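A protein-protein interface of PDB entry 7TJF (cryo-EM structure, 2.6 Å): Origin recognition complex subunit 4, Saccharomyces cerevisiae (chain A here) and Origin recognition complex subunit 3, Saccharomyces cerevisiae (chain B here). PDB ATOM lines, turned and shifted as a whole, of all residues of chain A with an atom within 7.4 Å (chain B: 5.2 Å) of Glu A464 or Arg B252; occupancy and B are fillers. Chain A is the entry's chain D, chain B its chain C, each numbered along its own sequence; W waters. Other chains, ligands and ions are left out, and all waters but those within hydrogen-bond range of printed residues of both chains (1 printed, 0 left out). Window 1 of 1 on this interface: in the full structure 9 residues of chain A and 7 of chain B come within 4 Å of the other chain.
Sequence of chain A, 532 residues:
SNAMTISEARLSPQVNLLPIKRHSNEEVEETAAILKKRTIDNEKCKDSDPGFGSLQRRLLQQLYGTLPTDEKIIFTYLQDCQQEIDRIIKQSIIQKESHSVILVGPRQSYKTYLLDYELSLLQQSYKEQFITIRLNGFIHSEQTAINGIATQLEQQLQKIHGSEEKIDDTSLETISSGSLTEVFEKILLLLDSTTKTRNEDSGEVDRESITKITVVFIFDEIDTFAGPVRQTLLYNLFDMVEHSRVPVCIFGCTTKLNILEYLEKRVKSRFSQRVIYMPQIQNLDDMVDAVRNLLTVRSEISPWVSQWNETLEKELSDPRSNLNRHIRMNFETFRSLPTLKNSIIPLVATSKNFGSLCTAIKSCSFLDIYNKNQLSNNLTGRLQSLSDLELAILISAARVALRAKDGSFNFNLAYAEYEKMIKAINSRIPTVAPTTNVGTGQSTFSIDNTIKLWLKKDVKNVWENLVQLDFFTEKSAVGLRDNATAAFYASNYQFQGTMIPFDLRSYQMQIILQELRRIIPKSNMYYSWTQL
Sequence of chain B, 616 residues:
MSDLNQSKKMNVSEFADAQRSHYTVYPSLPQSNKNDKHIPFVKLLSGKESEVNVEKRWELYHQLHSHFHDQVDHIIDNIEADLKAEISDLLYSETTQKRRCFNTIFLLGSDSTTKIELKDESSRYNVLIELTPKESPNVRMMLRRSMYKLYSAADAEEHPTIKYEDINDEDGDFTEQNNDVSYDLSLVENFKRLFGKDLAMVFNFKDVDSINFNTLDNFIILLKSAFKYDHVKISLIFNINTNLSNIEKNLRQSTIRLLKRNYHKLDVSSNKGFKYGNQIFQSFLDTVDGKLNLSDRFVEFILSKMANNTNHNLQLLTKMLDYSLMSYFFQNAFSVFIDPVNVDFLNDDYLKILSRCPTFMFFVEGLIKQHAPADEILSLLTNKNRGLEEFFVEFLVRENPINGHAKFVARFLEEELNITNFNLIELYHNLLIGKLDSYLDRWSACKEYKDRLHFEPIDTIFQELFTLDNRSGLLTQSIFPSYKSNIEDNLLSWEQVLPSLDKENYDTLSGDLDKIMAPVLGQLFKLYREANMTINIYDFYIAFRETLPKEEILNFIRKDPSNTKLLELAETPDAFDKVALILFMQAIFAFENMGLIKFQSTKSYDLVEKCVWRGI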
ATOM      1  N   PHE A 411      15.239  -3.276 -16.039  1.00  0.00           N
ATOM      2  CA  PHE A 411      14.335  -2.226 -15.581  1.00  0.00           C
ATOM      3  C   PHE A 411      12.935  -2.383 -16.165  1.00  0.00           C
ATOM      4  O   PHE A 411      11.941  -2.124 -15.477  1.00  0.00           O
ATOM      5  CB  PHE A 411      14.938  -0.871 -15.949  1.00  0.00           C
ATOM      6  CG  PHE A 411      14.108   0.308 -15.550  1.00  0.00           C
ATOM      7  CD1 PHE A 411      14.144   0.786 -14.253  1.00  0.00           C
ATOM      8  CD2 PHE A 411      13.332   0.977 -16.487  1.00  0.00           C
ATOM      9  CE1 PHE A 411      13.403   1.885 -13.886  1.00  0.00           C
ATOM     10  CE2 PHE A 411      12.582   2.078 -16.124  1.00  0.00           C
ATOM     11  CZ  PHE A 411      12.618   2.533 -14.822  1.00  0.00           C
ATOM     12  N   LYS A 457      10.080   7.525 -15.929  1.00  0.00           N
ATOM     13  CA  LYS A 457      11.138   8.500 -15.686  1.00  0.00           C
ATOM     14  C   LYS A 457      11.365   8.734 -14.199  1.00  0.00           C
ATOM     15  O   LYS A 457      12.496   9.002 -13.781  1.00  0.00           O
ATOM     16  CB  LYS A 457      10.803   9.819 -16.381  1.00  0.00           C
ATOM     17  CG  LYS A 457       9.555  10.505 -15.848  1.00  0.00           C
ATOM     18  CD  LYS A 457       9.303  11.818 -16.571  1.00  0.00           C
ATOM     19  CE  LYS A 457       8.057  12.513 -16.046  1.00  0.00           C
ATOM     20  NZ  LYS A 457       7.803  13.801 -16.749  1.00  0.00           N
ATOM     21  N   VAL A 459      10.643   6.310 -11.881  1.00  0.00           N
ATOM     22  CA  VAL A 459      11.115   5.034 -11.352  1.00  0.00           C
ATOM     23  C   VAL A 459      12.590   4.804 -11.698  1.00  0.00           C
ATOM     24  O   VAL A 459      13.271   4.038 -11.003  1.00  0.00           O
ATOM     25  CB  VAL A 459      10.119   3.954 -11.839  1.00  0.00           C
ATOM     26  CG1 VAL A 459      10.615   2.524 -11.695  1.00  0.00           C
ATOM     27  CG2 VAL A 459       8.819   4.078 -11.062  1.00  0.00           C
ATOM     28  N   LYS A 460      13.117   5.513 -12.708  1.00  0.00           N
ATOM     29  CA  LYS A 460      14.547   5.447 -13.031  1.00  0.00           C
ATOM     30  C   LYS A 460      15.425   5.909 -11.862  1.00  0.00           C
ATOM     31  O   LYS A 460      16.467   5.301 -11.581  1.00  0.00           O
ATOM     32  CB  LYS A 460      14.824   6.287 -14.281  1.00  0.00           C
ATOM     33  CG  LYS A 460      16.293   6.575 -14.578  1.00  0.00           C
ATOM     34  CD  LYS A 460      16.445   7.323 -15.892  1.00  0.00           C
ATOM     35  CE  LYS A 460      17.903   7.603 -16.225  1.00  0.00           C
ATOM     36  NZ  LYS A 460      18.518   8.565 -15.275  1.00  0.00           N
ATOM     37  N   ASN A 461      15.002   6.961 -11.155  1.00  0.00           N
ATOM     38  CA  ASN A 461      15.753   7.454 -10.000  1.00  0.00           C
ATOM     39  C   ASN A 461      15.736   6.458  -8.844  1.00  0.00           C
ATOM     40  O   ASN A 461      16.761   6.252  -8.179  1.00  0.00           O
ATOM     41  CB  ASN A 461      15.184   8.800  -9.557  1.00  0.00           C
ATOM     42  CG  ASN A 461      15.889   9.363  -8.345  1.00  0.00           C
ATOM     43  OD1 ASN A 461      16.982   9.913  -8.450  1.00  0.00           O
ATOM     44  ND2 ASN A 461      15.262   9.230  -7.182  1.00  0.00           N
ATOM     45  N   VAL A 462      14.582   5.828  -8.599  1.00  0.00           N
ATOM     46  CA  VAL A 462      14.468   4.786  -7.578  1.00  0.00           C
ATOM     47  C   VAL A 462      15.340   3.587  -7.941  1.00  0.00           C
ATOM     48  O   VAL A 462      15.994   2.988  -7.079  1.00  0.00           O
ATOM     49  CB  VAL A 462      12.981   4.407  -7.401  1.00  0.00           C
ATOM     50  CG1 VAL A 462      12.795   3.022  -6.785  1.00  0.00           C
ATOM     51  CG2 VAL A 462      12.270   5.455  -6.570  1.00  0.00           C
ATOM     52  N   TRP A 463      15.392   3.257  -9.234  1.00  0.00           N
ATOM     53  CA  TRP A 463      16.241   2.177  -9.730  1.00  0.00           C
ATOM     54  C   TRP A 463      17.721   2.471  -9.509  1.00  0.00           C
ATOM     55  O   TRP A 463      18.485   1.589  -9.096  1.00  0.00           O
ATOM     56  CB  TRP A 463      15.948   1.964 -11.214  1.00  0.00           C
ATOM     57  CG  TRP A 463      16.607   0.787 -11.823  1.00  0.00           C
ATOM     58  CD1 TRP A 463      17.778   0.772 -12.514  1.00  0.00           C
ATOM     59  CD2 TRP A 463      16.123  -0.557 -11.819  1.00  0.00           C
ATOM     60  NE1 TRP A 463      18.061  -0.502 -12.935  1.00  0.00           N
ATOM     61  CE2 TRP A 463      17.058  -1.337 -12.524  1.00  0.00           C
ATOM     62  CE3 TRP A 463      14.988  -1.176 -11.291  1.00  0.00           C
ATOM     63  CZ2 TRP A 463      16.898  -2.705 -12.709  1.00  0.00           C
ATOM     64  CZ3 TRP A 463      14.829  -2.532 -11.474  1.00  0.00           C
ATOM     65  CH2 TRP A 463      15.778  -3.282 -12.179  1.00  0.00           C
ATOM     66  N   GLU A 464      18.138   3.714  -9.769  1.00  0.00           N
ATOM     67  CA  GLU A 464      19.526   4.103  -9.533  1.00  0.00           C
ATOM     68  C   GLU A 464      19.861   4.105  -8.045  1.00  0.00           C
ATOM     69  O   GLU A 464      20.979   3.747  -7.656  1.00  0.00           O
ATOM     70  CB  GLU A 464      19.798   5.473 -10.152  1.00  0.00           C
ATOM     71  CG  GLU A 464      20.111   5.421 -11.639  1.00  0.00           C
ATOM     72  CD  GLU A 464      19.714   6.688 -12.373  1.00  0.00           C
ATOM     73  OE1 GLU A 464      19.167   7.606 -11.728  1.00  0.00           O
ATOM     74  OE2 GLU A 464      19.949   6.764 -13.595  1.00  0.00           O
ATOM     75  N   ASN A 465      18.903   4.494  -7.197  1.00  0.00           N
ATOM     76  CA  ASN A 465      19.129   4.443  -5.756  1.00  0.00           C
ATOM     77  C   ASN A 465      19.196   3.011  -5.236  1.00  0.00           C
ATOM     78  O   ASN A 465      19.925   2.737  -4.277  1.00  0.00           O
ATOM     79  CB  ASN A 465      18.041   5.225  -5.023  1.00  0.00           C
ATOM     80  CG  ASN A 465      18.096   6.706  -5.321  1.00  0.00           C
ATOM     81  OD1 ASN A 465      19.046   7.189  -5.932  1.00  0.00           O
ATOM     82  ND2 ASN A 465      17.077   7.435  -4.893  1.00  0.00           N
ATOM     83  N   LEU A 466      18.442   2.092  -5.843  1.00  0.00           N
ATOM     84  CA  LEU A 466      18.522   0.691  -5.446  1.00  0.00           C
ATOM     85  C   LEU A 466      19.814   0.042  -5.926  1.00  0.00           C
ATOM     86  O   LEU A 466      20.332  -0.864  -5.265  1.00  0.00           O
ATOM     87  CB  LEU A 466      17.318  -0.083  -5.980  1.00  0.00           C
ATOM     88  CG  LEU A 466      15.981   0.146  -5.274  1.00  0.00           C
ATOM     89  CD1 LEU A 466      14.850  -0.500  -6.054  1.00  0.00           C
ATOM     90  CD2 LEU A 466      16.021  -0.371  -3.842  1.00  0.00           C
ATOM     91  N   VAL A 467      20.324   0.466  -7.086  1.00  0.00           N
ATOM     92  CA  VAL A 467      21.634   0.005  -7.538  1.00  0.00           C
ATOM     93  C   VAL A 467      22.731   0.541  -6.621  1.00  0.00           C
ATOM     94  O   VAL A 467      23.649  -0.194  -6.234  1.00  0.00           O
ATOM     95  CB  VAL A 467      21.853   0.406  -9.012  1.00  0.00           C
ATOM     96  CG1 VAL A 467      23.322   0.316  -9.412  1.00  0.00           C
ATOM     97  CG2 VAL A 467      21.011  -0.469  -9.925  1.00  0.00           C
ATOM     98  N   GLN A 468      22.623   1.816  -6.224  1.00  0.00           N
ATOM     99  CA  GLN A 468      23.639   2.453  -5.390  1.00  0.00           C
ATOM    100  C   GLN A 468      23.689   1.859  -3.985  1.00  0.00           C
ATOM    101  O   GLN A 468      24.773   1.736  -3.405  1.00  0.00           O
ATOM    102  CB  GLN A 468      23.382   3.962  -5.331  1.00  0.00           C
ATOM    103  CG  GLN A 468      24.418   4.767  -4.565  1.00  0.00           C
ATOM    104  CD  GLN A 468      24.624   6.155  -5.143  1.00  0.00           C
ATOM    105  OE1 GLN A 468      24.206   7.153  -4.556  1.00  0.00           O
ATOM    106  NE2 GLN A 468      25.273   6.224  -6.299  1.00  0.00           N
ATOM    107  N   LEU A 469      22.544   1.447  -3.439  1.00  0.00           N
ATOM    108  CA  LEU A 469      22.487   0.838  -2.114  1.00  0.00           C
ATOM    109  C   LEU A 469      22.785  -0.656  -2.122  1.00  0.00           C
ATOM    110  O   LEU A 469      22.536  -1.313  -1.105  1.00  0.00           O
ATOM    111  CB  LEU A 469      21.116   1.078  -1.479  1.00  0.00           C
ATOM    112  CG  LEU A 469      20.915   2.431  -0.801  1.00  0.00           C
ATOM    113  CD1 LEU A 469      19.442   2.694  -0.581  1.00  0.00           C
ATOM    114  CD2 LEU A 469      21.682   2.491   0.508  1.00  0.00           C
ATOM    115  N   ASP A 470      23.281  -1.187  -3.248  1.00  0.00           N
ATOM    116  CA  ASP A 470      23.740  -2.572  -3.413  1.00  0.00           C
ATOM    117  C   ASP A 470      22.600  -3.575  -3.185  1.00  0.00           C
ATOM    118  O   ASP A 470      22.803  -4.697  -2.714  1.00  0.00           O
ATOM    119  CB  ASP A 470      24.959  -2.856  -2.514  1.00  0.00           C
ATOM    120  CG  ASP A 470      25.726  -4.111  -2.917  1.00  0.00           C
ATOM    121  OD1 ASP A 470      25.858  -4.371  -4.132  1.00  0.00           O
ATOM    122  OD2 ASP A 470      26.191  -4.838  -2.014  1.00  0.00           O
ATOM    123  N   PHE A 472      20.784  -4.295  -5.977  1.00  0.00           N
ATOM    124  CA  PHE A 472      20.961  -4.945  -7.268  1.00  0.00           C
ATOM    125  C   PHE A 472      22.443  -5.062  -7.585  1.00  0.00           C
ATOM    126  O   PHE A 472      23.280  -4.355  -7.018  1.00  0.00           O
ATOM    127  CB  PHE A 472      20.277  -4.177  -8.410  1.00  0.00           C
ATOM    128  CG  PHE A 472      18.812  -3.931  -8.213  1.00  0.00           C
ATOM    129  CD1 PHE A 472      18.012  -4.830  -7.521  1.00  0.00           C
ATOM    130  CD2 PHE A 472      18.222  -2.802  -8.764  1.00  0.00           C
ATOM    131  CE1 PHE A 472      16.662  -4.587  -7.360  1.00  0.00           C
ATOM    132  CE2 PHE A 472      16.876  -2.561  -8.610  1.00  0.00           C
ATOM    133  CZ  PHE A 472      16.094  -3.455  -7.907  1.00  0.00           C
ATOM    134  N   PHE A 502      20.112   1.972 -20.207  1.00  0.00           N
ATOM    135  CA  PHE A 502      20.021   1.528 -18.816  1.00  0.00           C
ATOM    136  C   PHE A 502      18.846   0.585 -18.575  1.00  0.00           C
ATOM    137  O   PHE A 502      18.894  -0.230 -17.648  1.00  0.00           O
ATOM    138  CB  PHE A 502      19.927   2.744 -17.884  1.00  0.00           C
ATOM    139  CG  PHE A 502      18.514   3.173 -17.576  1.00  0.00           C
ATOM    140  CD1 PHE A 502      17.759   3.846 -18.526  1.00  0.00           C
ATOM    141  CD2 PHE A 502      17.942   2.904 -16.338  1.00  0.00           C
ATOM    142  CE1 PHE A 502      16.460   4.235 -18.251  1.00  0.00           C
ATOM    143  CE2 PHE A 502      16.641   3.284 -16.062  1.00  0.00           C
ATOM    144  CZ  PHE A 502      15.902   3.951 -17.021  1.00  0.00           C
ATOM    145  N   ARG A 505      19.903  -3.309 -19.135  1.00  0.00           N
ATOM    146  CA  ARG A 505      21.014  -3.930 -18.422  1.00  0.00           C
ATOM    147  C   ARG A 505      20.533  -5.090 -17.561  1.00  0.00           C
ATOM    148  O   ARG A 505      19.570  -4.957 -16.802  1.00  0.00           O
ATOM    149  CB  ARG A 505      21.727  -2.903 -17.547  1.00  0.00           C
ATOM    150  CG  ARG A 505      22.215  -1.670 -18.272  1.00  0.00           C
ATOM    151  CD  ARG A 505      23.442  -1.120 -17.572  1.00  0.00           C
ATOM    152  NE  ARG A 505      23.188   0.103 -16.825  1.00  0.00           N
ATOM    153  CZ  ARG A 505      23.288   1.324 -17.331  1.00  0.00           C
ATOM    154  NH1 ARG A 505      23.614   1.522 -18.598  1.00  0.00           N
ATOM    155  NH2 ARG A 505      23.063   2.372 -16.544  1.00  0.00           N
ATOM    156  N   TYR A 507      20.505  -7.507 -14.457  1.00  0.00           N
ATOM    157  CA  TYR A 507      20.811  -7.356 -13.045  1.00  0.00           C
ATOM    158  C   TYR A 507      20.400  -8.617 -12.305  1.00  0.00           C
ATOM    159  O   TYR A 507      19.587  -9.407 -12.786  1.00  0.00           O
ATOM    160  CB  TYR A 507      20.105  -6.142 -12.431  1.00  0.00           C
ATOM    161  CG  TYR A 507      20.804  -4.829 -12.676  1.00  0.00           C
ATOM    162  CD1 TYR A 507      21.849  -4.418 -11.858  1.00  0.00           C
ATOM    163  CD2 TYR A 507      20.409  -3.993 -13.713  1.00  0.00           C
ATOM    164  CE1 TYR A 507      22.488  -3.215 -12.070  1.00  0.00           C
ATOM    165  CE2 TYR A 507      21.043  -2.784 -13.934  1.00  0.00           C
ATOM    166  CZ  TYR A 507      22.082  -2.402 -13.111  1.00  0.00           C
ATOM    167  OH  TYR A 507      22.720  -1.203 -13.323  1.00  0.00           O
ATOM    168  N   ASN B 214      29.342   6.416 -18.574  1.00  0.00           N
ATOM    169  CA  ASN B 214      29.718   6.152 -17.188  1.00  0.00           C
ATOM    170  C   ASN B 214      30.963   6.940 -16.797  1.00  0.00           C
ATOM    171  O   ASN B 214      31.016   7.534 -15.710  1.00  0.00           O
ATOM    172  CB  ASN B 214      29.937   4.650 -16.990  1.00  0.00           C
ATOM    173  CG  ASN B 214      30.654   4.331 -15.697  1.00  0.00           C
ATOM    174  OD1 ASN B 214      30.068   4.392 -14.619  1.00  0.00           O
ATOM    175  ND2 ASN B 214      31.932   3.979 -15.801  1.00  0.00           N
ATOM    176  N   ASP B 217      29.919  10.674 -16.557  1.00  0.00           N
ATOM    177  CA  ASP B 217      29.187  10.888 -15.309  1.00  0.00           C
ATOM    178  C   ASP B 217      30.123  10.937 -14.109  1.00  0.00           C
ATOM    179  O   ASP B 217      30.010  11.826 -13.251  1.00  0.00           O
ATOM    180  CB  ASP B 217      28.150   9.782 -15.117  1.00  0.00           C
ATOM    181  CG  ASP B 217      26.843  10.298 -14.559  1.00  0.00           C
ATOM    182  OD1 ASP B 217      26.865  10.870 -13.450  1.00  0.00           O
ATOM    183  OD2 ASP B 217      25.793  10.115 -15.205  1.00  0.00           O
ATOM    184  N   ASN B 218      31.070   9.993 -14.042  1.00  0.00           N
ATOM    185  CA  ASN B 218      32.021   9.988 -12.937  1.00  0.00           C
ATOM    186  C   ASN B 218      32.962  11.186 -12.993  1.00  0.00           C
ATOM    187  O   ASN B 218      33.370  11.692 -11.947  1.00  0.00           O
ATOM    188  CB  ASN B 218      32.804   8.676 -12.923  1.00  0.00           C
ATOM    189  CG  ASN B 218      31.952   7.495 -12.504  1.00  0.00           C
ATOM    190  OD1 ASN B 218      31.940   6.459 -13.165  1.00  0.00           O
ATOM    191  ND2 ASN B 218      31.225   7.651 -11.405  1.00  0.00           N
ATOM    192  N   ILE B 221      30.938  14.137 -11.609  1.00  0.00           N
ATOM    193  CA  ILE B 221      30.874  13.980 -10.157  1.00  0.00           C
ATOM    194  C   ILE B 221      32.222  14.310  -9.513  1.00  0.00           C
ATOM    195  O   ILE B 221      32.276  14.904  -8.427  1.00  0.00           O
ATOM    196  CB  ILE B 221      30.368  12.562  -9.818  1.00  0.00           C
ATOM    197  CG1 ILE B 221      28.880  12.478 -10.142  1.00  0.00           C
ATOM    198  CG2 ILE B 221      30.586  12.183  -8.361  1.00  0.00           C
ATOM    199  CD1 ILE B 221      28.368  11.083 -10.275  1.00  0.00           C
ATOM    200  N   ASN B 250      21.118   8.535 -20.713  1.00  0.00           N
ATOM    201  CA  ASN B 250      22.363   7.840 -20.430  1.00  0.00           C
ATOM    202  C   ASN B 250      23.068   8.369 -19.190  1.00  0.00           C
ATOM    203  O   ASN B 250      23.972   7.701 -18.679  1.00  0.00           O
ATOM    204  CB  ASN B 250      23.309   7.938 -21.632  1.00  0.00           C
ATOM    205  CG  ASN B 250      22.782   7.203 -22.845  1.00  0.00           C
ATOM    206  OD1 ASN B 250      22.063   6.214 -22.721  1.00  0.00           O
ATOM    207  ND2 ASN B 250      23.134   7.686 -24.030  1.00  0.00           N
ATOM    208  N   LEU B 251      22.684   9.543 -18.704  1.00  0.00           N
ATOM    209  CA  LEU B 251      23.213  10.094 -17.468  1.00  0.00           C
ATOM    210  C   LEU B 251      22.314   9.717 -16.297  1.00  0.00           C
ATOM    211  O   LEU B 251      21.110   9.496 -16.450  1.00  0.00           O
ATOM    212  CB  LEU B 251      23.328  11.616 -17.562  1.00  0.00           C
ATOM    213  CG  LEU B 251      24.441  12.224 -18.418  1.00  0.00           C
ATOM    214  CD1 LEU B 251      24.591  13.694 -18.084  1.00  0.00           C
ATOM    215  CD2 LEU B 251      25.762  11.488 -18.237  1.00  0.00           C
ATOM    216  N   ARG B 252      22.916   9.645 -15.114  1.00  0.00           N
ATOM    217  CA  ARG B 252      22.154   9.360 -13.908  1.00  0.00           C
ATOM    218  C   ARG B 252      21.374  10.591 -13.459  1.00  0.00           C
ATOM    219  O   ARG B 252      21.728  11.728 -13.779  1.00  0.00           O
ATOM    220  CB  ARG B 252      23.083   8.852 -12.804  1.00  0.00           C
ATOM    221  CG  ARG B 252      23.628   7.464 -13.111  1.00  0.00           C
ATOM    222  CD  ARG B 252      24.294   6.799 -11.918  1.00  0.00           C
ATOM    223  NE  ARG B 252      25.473   7.516 -11.450  1.00  0.00           N
ATOM    224  CZ  ARG B 252      26.692   7.342 -11.945  1.00  0.00           C
ATOM    225  NH1 ARG B 252      26.923   6.489 -12.932  1.00  0.00           N
ATOM    226  NH2 ARG B 252      27.704   8.033 -11.435  1.00  0.00           N
ATOM    227  N   GLN B 253      20.286  10.341 -12.718  1.00  0.00           N
ATOM    228  CA  GLN B 253      19.304  11.380 -12.413  1.00  0.00           C
ATOM    229  C   GLN B 253      19.864  12.452 -11.485  1.00  0.00           C
ATOM    230  O   GLN B 253      19.483  13.624 -11.597  1.00  0.00           O
ATOM    231  CB  GLN B 253      18.055  10.744 -11.800  1.00  0.00           C
ATOM    232  CG  GLN B 253      16.801  11.600 -11.861  1.00  0.00           C
ATOM    233  CD  GLN B 253      16.428  11.997 -13.274  1.00  0.00           C
ATOM    234  OE1 GLN B 253      16.409  11.165 -14.180  1.00  0.00           O
ATOM    235  NE2 GLN B 253      16.127  13.274 -13.468  1.00  0.00           N
ATOM    236  N   SER B 254      20.762  12.075 -10.570  1.00  0.00           N
ATOM    237  CA  SER B 254      21.412  13.062  -9.716  1.00  0.00           C
ATOM    238  C   SER B 254      22.340  13.972 -10.513  1.00  0.00           C
ATOM    239  O   SER B 254      22.443  15.165 -10.207  1.00  0.00           O
ATOM    240  CB  SER B 254      22.177  12.365  -8.590  1.00  0.00           C
ATOM    241  OG  SER B 254      23.093  11.416  -9.103  1.00  0.00           O
ATOM    242  N   THR B 255      22.995  13.440 -11.548  1.00  0.00           N
ATOM    243  CA  THR B 255      23.820  14.270 -12.422  1.00  0.00           C
ATOM    244  C   THR B 255      22.968  15.245 -13.231  1.00  0.00           C
ATOM    245  O   THR B 255      23.373  16.391 -13.455  1.00  0.00           O
ATOM    246  CB  THR B 255      24.655  13.388 -13.351  1.00  0.00           C
ATOM    247  OG1 THR B 255      25.223  12.305 -12.605  1.00  0.00           O
ATOM    248  CG2 THR B 255      25.779  14.189 -13.996  1.00  0.00           C
ATOM    249  N   ILE B 256      21.782  14.808 -13.664  1.00  0.00           N
ATOM    250  CA  ILE B 256      20.866  15.690 -14.383  1.00  0.00           C
ATOM    251  C   ILE B 256      20.343  16.786 -13.460  1.00  0.00           C
ATOM    252  O   ILE B 256      20.220  17.949 -13.865  1.00  0.00           O
ATOM    253  CB  ILE B 256      19.723  14.867 -15.009  1.00  0.00           C
ATOM    254  CG1 ILE B 256      20.287  13.834 -15.981  1.00  0.00           C
ATOM    255  CG2 ILE B 256      18.744  15.756 -15.762  1.00  0.00           C
ATOM    256  CD1 ILE B 256      19.450  12.591 -16.071  1.00  0.00           C
HETATM  257  O   HOH W   1      20.508   9.238  -9.966  1.00  0.00           O
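NH2 of Arg B252 lies within salt-bridge range of OD1 of Asp B217 (3.6 Å).
OD1 of Asn A465 lies close to O of Asn A461, at 3.3 Å.
The side-chain carboxylate (OE2) of Glu A464 is in salt-bridge range of the side-chain amino group (NZ) of Lys A460.
Of the 11 printed residues of chain B, 3 touch a printed residue of chain A.
Among the printed residues, no Asp or Glu carboxylate lies within 4 Å of a Lys or Arg side-chain nitrogen of the other chain.
Water W1 lies within hydrogen-bond range of OE1 of Glu A464 (2.8 Å), N of Ser B254 (2.9 Å) and N of Gln B253 (3.0 Å).
Among the printed residues, pairs that only touch across the chains: Lys A460 with Arg B252 (3.9 Å), Lys A460 with Gln B253 (3.5 Å), Asn A461 with Gln B253 (3.6 Å) and Glu A464 with Arg B252 (3.4 Å).
The side-chain amino group (NZ) of Lys A460 sits at hydrogen-bond distance from the backbone carbonyl oxygen (O) of Leu B251 (3.0 Å).
The backbone NH (N) of Gln B253 lies within hydrogen-bond range of the side-chain carboxylate (OE1) of Glu A464 (3.1 Å).
Printed residues of chain B within 4 Å of Lys A460: Leu B251 (3.0 Å), Arg B252 (3.9 Å) and Gln B253 (3.5 Å).
Of chain B, only Arg B252 (3.4 Å) and Gln B253 (3.1 Å) come within 4 Å of Glu A464.
Arg B252 touches two residues of chain A.
Printed residues of chain A within 4 Å of Gln B253: Lys A460, Asn A461 and Glu A464.
The nearest printed residue of chain A that does not touch Gln B253 is Lys A457 (4.5 Å).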
